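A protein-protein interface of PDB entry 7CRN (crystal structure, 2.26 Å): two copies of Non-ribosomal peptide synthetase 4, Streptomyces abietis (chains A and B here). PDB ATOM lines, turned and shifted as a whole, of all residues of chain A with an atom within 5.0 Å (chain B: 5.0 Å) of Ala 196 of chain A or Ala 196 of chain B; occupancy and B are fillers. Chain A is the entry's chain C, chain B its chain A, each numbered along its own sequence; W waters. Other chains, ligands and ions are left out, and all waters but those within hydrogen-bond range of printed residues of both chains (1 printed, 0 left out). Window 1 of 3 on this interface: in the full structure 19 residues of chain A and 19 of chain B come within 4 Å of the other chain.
The side-chain amide oxygen (OD1) of Asn 197 of chain B is in hydrogen-bond range of the guanidinium group (NH2) of Arg 199 of chain A, 3.4 Å away. The side-chain amide oxygen of Asn 197 of chain A is in hydrogen-bond range of the guanidinium group of Arg 199 of chain B (3.4 Å). The guanidinium group (NH1) of Arg 199 of chain B lies within hydrogen-bond range of the side-chain hydroxyl (OG) of Ser 200 of chain A, 3.2 Å away. The side-chain hydroxyl of Ser 200 of chain B lies within hydrogen-bond range of the guanidinium group of Arg 199 of chain A, 3.1 Å away.
OG of Ser 200 of chain B lies within hydrogen-bond range of O of Asn 197 of chain B (2.8 Å). The backbone carbonyl oxygen (O) of Asn 197 of chain A sits at hydrogen-bond distance from the side-chain hydroxyl (OG) of Ser 200 of chain A (2.8 Å).
Phe 195 of chain A touches Ala 196 of chain B (CD2 to CB, 3.6 Å). Ala 196 of chain A touches Phe 195 of chain B. CB of Ala 196 of chain A touches CA of Ala 196 of chain B (3.8 Å).
Of chain B, only Phe 195 and Ala 196 come within 4 Å of Ala 196 of chain A. Ala 196 of chain B touches just these residues of chain A: Phe 195 and Ala 196. Of the printed residues of chain A, Asn 197 of chain B touches Arg 199. Of the printed residues of chain B, Asn 197 of chain A touches Arg 199 (3.4 Å). Of the printed residues of chain B, Ser 200 of chain A touches Arg 199 (3.2 Å). Of the printed residues of chain A, Arg 199 of chain B touches Asn 197 and Ser 200. Printed residues of chain A within 4 Å of Ser 200 of chain B: Arg 199. Ser 198 of chain B touches none of the printed residues of chain A. Val 194 of chain B touches none of the printed residues of chain A. The nearest residue of chain A that does not touch Ala 196 of chain B is Arg 199 of chain A (4.1 Å). The nearest printed residue of chain B that does not touch Ser 200 of chain A is Ser 200 of chain B (4.4 Å).
Hydrophobic or aromatic side chains of chain B within 4 Å of the printed part of chain A: Phe 195 and Ala 196. Hydrophobic or aromatic side chains of chain A that line the printed part of chain B: Phe 195 and Ala 196. Among the printed residues, no Asp or Glu carboxylate lies within 4 Å of a Lys or Arg side-chain nitrogen of the other chain.
Phe 195 of chain A touches Ala 196 of chain B, and with the chains exchanged Ala 196 of chain A touches Phe 195 of chain B. Ala 196 of chain A touches its own counterpart, Ala 196 of chain B. Asn 197 of chain A touches Arg 199 of chain B, and with the chains exchanged Arg 199 of chain A touches Asn 197 of chain B. Arg 199 of chain A touches Ser 200 of chain B, and with the chains exchanged Ser 200 of chain A touches Arg 199 of chain B. 9 positions are printed for both chains. Of the 7 pairs that touch across the chains among the printed residues, 7 have their exchanged pair printed and touching as well.
Water W1 lies within hydrogen-bond range of NH2 of Arg 199 of chain B (2.7 Å), OD1 of Asn 193 of chain A (2.9 Å) and N of Asn 197 of chain A (3.3 Å).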
ATOM      1  N   ALA A 192      -4.106  16.601 -29.006  1.00  0.00           N
ATOM      2  CA  ALA A 192      -5.148  15.614 -28.717  1.00  0.00           C
ATOM      3  C   ALA A 192      -5.963  16.005 -27.483  1.00  0.00           C
ATOM      4  O   ALA A 192      -7.195  15.880 -27.469  1.00  0.00           O
ATOM      5  CB  ALA A 192      -4.521  14.235 -28.525  1.00  0.00           C
ATOM      6  N   ASN A 193      -5.283  16.464 -26.431  1.00  0.00           N
ATOM      7  CA  ASN A 193      -5.952  16.896 -25.206  1.00  0.00           C
ATOM      8  C   ASN A 193      -6.928  18.030 -25.488  1.00  0.00           C
ATOM      9  O   ASN A 193      -8.074  18.022 -25.017  1.00  0.00           O
ATOM     10  CB  ASN A 193      -4.902  17.326 -24.178  1.00  0.00           C
ATOM     11  CG  ASN A 193      -5.503  17.616 -22.810  1.00  0.00           C
ATOM     12  OD1 ASN A 193      -6.535  17.060 -22.449  1.00  0.00           O
ATOM     13  ND2 ASN A 193      -4.856  18.492 -22.048  1.00  0.00           N
ATOM     14  N   VAL A 194      -6.475  19.034 -26.238  1.00  0.00           N
ATOM     15  CA  VAL A 194      -7.323  20.173 -26.566  1.00  0.00           C
ATOM     16  C   VAL A 194      -8.510  19.728 -27.411  1.00  0.00           C
ATOM     17  O   VAL A 194      -9.632  20.214 -27.231  1.00  0.00           O
ATOM     18  CB  VAL A 194      -6.490  21.265 -27.264  1.00  0.00           C
ATOM     19  CG1 VAL A 194      -7.387  22.279 -27.937  1.00  0.00           C
ATOM     20  CG2 VAL A 194      -5.581  21.944 -26.248  1.00  0.00           C
ATOM     21  N   PHE A 195      -8.290  18.791 -28.335  1.00  0.00           N
ATOM     22  CA  PHE A 195      -9.398  18.307 -29.154  1.00  0.00           C
ATOM     23  C   PHE A 195     -10.444  17.592 -28.301  1.00  0.00           C
ATOM     24  O   PHE A 195     -11.649  17.812 -28.462  1.00  0.00           O
ATOM     25  CB  PHE A 195      -8.883  17.386 -30.261  1.00  0.00           C
ATOM     26  CG  PHE A 195      -9.976  16.848 -31.139  1.00  0.00           C
ATOM     27  CD1 PHE A 195     -10.523  17.631 -32.142  1.00  0.00           C
ATOM     28  CD2 PHE A 195     -10.480  15.573 -30.939  1.00  0.00           C
ATOM     29  CE1 PHE A 195     -11.552  17.149 -32.942  1.00  0.00           C
ATOM     30  CE2 PHE A 195     -11.511  15.083 -31.735  1.00  0.00           C
ATOM     31  CZ  PHE A 195     -12.044  15.873 -32.736  1.00  0.00           C
ATOM     32  N   ALA A 196      -9.996  16.719 -27.390  1.00  0.00           N
ATOM     33  CA  ALA A 196     -10.920  16.029 -26.489  1.00  0.00           C
ATOM     34  C   ALA A 196     -11.708  17.015 -25.626  1.00  0.00           C
ATOM     35  O   ALA A 196     -12.928  16.871 -25.458  1.00  0.00           O
ATOM     36  CB  ALA A 196     -10.154  15.037 -25.613  1.00  0.00           C
ATOM     37  N   ASN A 197     -11.031  18.023 -25.069  1.00  0.00           N
ATOM     38  CA  ASN A 197     -11.724  19.019 -24.252  1.00  0.00           C
ATOM     39  C   ASN A 197     -12.751  19.792 -25.081  1.00  0.00           C
ATOM     40  O   ASN A 197     -13.912  19.981 -24.664  1.00  0.00           O
ATOM     41  CB  ASN A 197     -10.701  19.976 -23.638  1.00  0.00           C
ATOM     42  CG  ASN A 197     -11.299  20.850 -22.566  1.00  0.00           C
ATOM     43  OD1 ASN A 197     -11.684  20.362 -21.508  1.00  0.00           O
ATOM     44  ND2 ASN A 197     -11.382  22.151 -22.830  1.00  0.00           N
ATOM     45  N   SER A 198     -12.339  20.241 -26.269  1.00  0.00           N
ATOM     46  CA  SER A 198     -13.239  20.993 -27.131  1.00  0.00           C
ATOM     47  C   SER A 198     -14.458  20.164 -27.480  1.00  0.00           C
ATOM     48  O   SER A 198     -15.581  20.682 -27.518  1.00  0.00           O
ATOM     49  CB  SER A 198     -12.500  21.420 -28.402  1.00  0.00           C
ATOM     50  OG  SER A 198     -11.429  22.304 -28.099  1.00  0.00           O
ATOM     51  N   ARG A 199     -14.260  18.862 -27.692  1.00  0.00           N
ATOM     52  CA  ARG A 199     -15.389  17.984 -27.959  1.00  0.00           C
ATOM     53  C   ARG A 199     -16.302  17.867 -26.747  1.00  0.00           C
ATOM     54  O   ARG A 199     -17.523  17.775 -26.901  1.00  0.00           O
ATOM     55  CB  ARG A 199     -14.892  16.602 -28.379  1.00  0.00           C
ATOM     56  CG  ARG A 199     -14.692  16.459 -29.869  1.00  0.00           C
ATOM     57  CD  ARG A 199     -15.023  15.056 -30.314  1.00  0.00           C
ATOM     58  NE  ARG A 199     -16.463  14.839 -30.322  1.00  0.00           N
ATOM     59  CZ  ARG A 199     -17.048  13.750 -30.806  1.00  0.00           C
ATOM     60  NH1 ARG A 199     -18.369  13.640 -30.769  1.00  0.00           N
ATOM     61  NH2 ARG A 199     -16.311  12.774 -31.325  1.00  0.00           N
ATOM     62  N   SER A 200     -15.739  17.898 -25.542  1.00  0.00           N
ATOM     63  CA  SER A 200     -16.608  17.827 -24.374  1.00  0.00           C
ATOM     64  C   SER A 200     -17.366  19.122 -24.128  1.00  0.00           C
ATOM     65  O   SER A 200     -18.270  19.134 -23.288  1.00  0.00           O
ATOM     66  CB  SER A 200     -15.805  17.466 -23.126  1.00  0.00           C
ATOM     67  OG  SER A 200     -15.168  18.610 -22.582  1.00  0.00           O
ATOM     68  N   ALA B 192      -6.570   8.202 -29.161  1.00  0.00           N
ATOM     69  CA  ALA B 192      -6.963   9.598 -28.963  1.00  0.00           C
ATOM     70  C   ALA B 192      -8.397   9.838 -29.428  1.00  0.00           C
ATOM     71  O   ALA B 192      -9.174  10.532 -28.760  1.00  0.00           O
ATOM     72  CB  ALA B 192      -6.002  10.527 -29.702  1.00  0.00           C
ATOM     73  N   ASN B 193      -8.758   9.276 -30.583  1.00  0.00           N
ATOM     74  CA  ASN B 193     -10.111   9.416 -31.113  1.00  0.00           C
ATOM     75  C   ASN B 193     -11.141   8.875 -30.131  1.00  0.00           C
ATOM     76  O   ASN B 193     -12.149   9.530 -29.836  1.00  0.00           O
ATOM     77  CB  ASN B 193     -10.204   8.676 -32.448  1.00  0.00           C
ATOM     78  CG  ASN B 193     -11.485   8.974 -33.193  1.00  0.00           C
ATOM     79  OD1 ASN B 193     -12.059  10.045 -33.040  1.00  0.00           O
ATOM     80  ND2 ASN B 193     -11.940   8.024 -34.006  1.00  0.00           N
ATOM     81  N   VAL B 194     -10.877   7.674 -29.629  1.00  0.00           N
ATOM     82  CA  VAL B 194     -11.762   7.022 -28.676  1.00  0.00           C
ATOM     83  C   VAL B 194     -11.909   7.858 -27.412  1.00  0.00           C
ATOM     84  O   VAL B 194     -13.006   7.985 -26.869  1.00  0.00           O
ATOM     85  CB  VAL B 194     -11.251   5.619 -28.299  1.00  0.00           C
ATOM     86  CG1 VAL B 194     -11.958   5.113 -27.051  1.00  0.00           C
ATOM     87  CG2 VAL B 194     -11.446   4.654 -29.460  1.00  0.00           C
ATOM     88  N   PHE B 195     -10.803   8.428 -26.943  1.00  0.00           N
ATOM     89  CA  PHE B 195     -10.845   9.249 -25.736  1.00  0.00           C
ATOM     90  C   PHE B 195     -11.678  10.510 -25.953  1.00  0.00           C
ATOM     91  O   PHE B 195     -12.514  10.868 -25.114  1.00  0.00           O
ATOM     92  CB  PHE B 195      -9.431   9.607 -25.291  1.00  0.00           C
ATOM     93  CG  PHE B 195      -9.397  10.425 -24.044  1.00  0.00           C
ATOM     94  CD1 PHE B 195      -9.556   9.822 -22.807  1.00  0.00           C
ATOM     95  CD2 PHE B 195      -9.249  11.800 -24.106  1.00  0.00           C
ATOM     96  CE1 PHE B 195      -9.550  10.578 -21.644  1.00  0.00           C
ATOM     97  CE2 PHE B 195      -9.243  12.563 -22.946  1.00  0.00           C
ATOM     98  CZ  PHE B 195      -9.394  11.946 -21.714  1.00  0.00           C
ATOM     99  N   ALA B 196     -11.457  11.200 -27.074  1.00  0.00           N
ATOM    100  CA  ALA B 196     -12.250  12.387 -27.385  1.00  0.00           C
ATOM    101  C   ALA B 196     -13.737  12.056 -27.475  1.00  0.00           C
ATOM    102  O   ALA B 196     -14.582  12.792 -26.947  1.00  0.00           O
ATOM    103  CB  ALA B 196     -11.756  13.021 -28.688  1.00  0.00           C
ATOM    104  N   ASN B 197     -14.079  10.948 -28.139  1.00  0.00           N
ATOM    105  CA  ASN B 197     -15.484  10.567 -28.259  1.00  0.00           C
ATOM    106  C   ASN B 197     -16.093  10.270 -26.889  1.00  0.00           C
ATOM    107  O   ASN B 197     -17.181  10.769 -26.546  1.00  0.00           O
ATOM    108  CB  ASN B 197     -15.612   9.357 -29.184  1.00  0.00           C
ATOM    109  CG  ASN B 197     -17.050   9.071 -29.571  1.00  0.00           C
ATOM    110  OD1 ASN B 197     -17.702   9.891 -30.218  1.00  0.00           O
ATOM    111  ND2 ASN B 197     -17.551   7.906 -29.177  1.00  0.00           N
ATOM    112  N   SER B 198     -15.382   9.483 -26.075  1.00  0.00           N
ATOM    113  CA  SER B 198     -15.884   9.138 -24.751  1.00  0.00           C
ATOM    114  C   SER B 198     -16.090  10.386 -23.913  1.00  0.00           C
ATOM    115  O   SER B 198     -17.077  10.495 -23.177  1.00  0.00           O
ATOM    116  CB  SER B 198     -14.903   8.192 -24.057  1.00  0.00           C
ATOM    117  OG  SER B 198     -14.692   7.021 -24.834  1.00  0.00           O
ATOM    118  N   ARG B 199     -15.190  11.364 -24.054  1.00  0.00           N
ATOM    119  CA  ARG B 199     -15.356  12.627 -23.349  1.00  0.00           C
ATOM    120  C   ARG B 199     -16.579  13.377 -23.847  1.00  0.00           C
ATOM    121  O   ARG B 199     -17.236  14.076 -23.070  1.00  0.00           O
ATOM    122  CB  ARG B 199     -14.111  13.485 -23.518  1.00  0.00           C
ATOM    123  CG  ARG B 199     -13.095  13.277 -22.432  1.00  0.00           C
ATOM    124  CD  ARG B 199     -12.375  14.560 -22.147  1.00  0.00           C
ATOM    125  NE  ARG B 199     -13.207  15.447 -21.350  1.00  0.00           N
ATOM    126  CZ  ARG B 199     -12.776  16.584 -20.823  1.00  0.00           C
ATOM    127  NH1 ARG B 199     -13.600  17.333 -20.107  1.00  0.00           N
ATOM    128  NH2 ARG B 199     -11.518  16.966 -21.017  1.00  0.00           N
ATOM    129  N   SER B 200     -16.897  13.251 -25.133  1.00  0.00           N
ATOM    130  CA  SER B 200     -18.112  13.899 -25.605  1.00  0.00           C
ATOM    131  C   SER B 200     -19.364  13.161 -25.158  1.00  0.00           C
ATOM    132  O   SER B 200     -20.462  13.706 -25.308  1.00  0.00           O
ATOM    133  CB  SER B 200     -18.110  14.034 -27.129  1.00  0.00           C
ATOM    134  OG  SER B 200     -18.570  12.844 -27.752  1.00  0.00           O
HETATM  135  O   HOH W   1      -9.381  16.458 -22.656  1.00  0.00           O
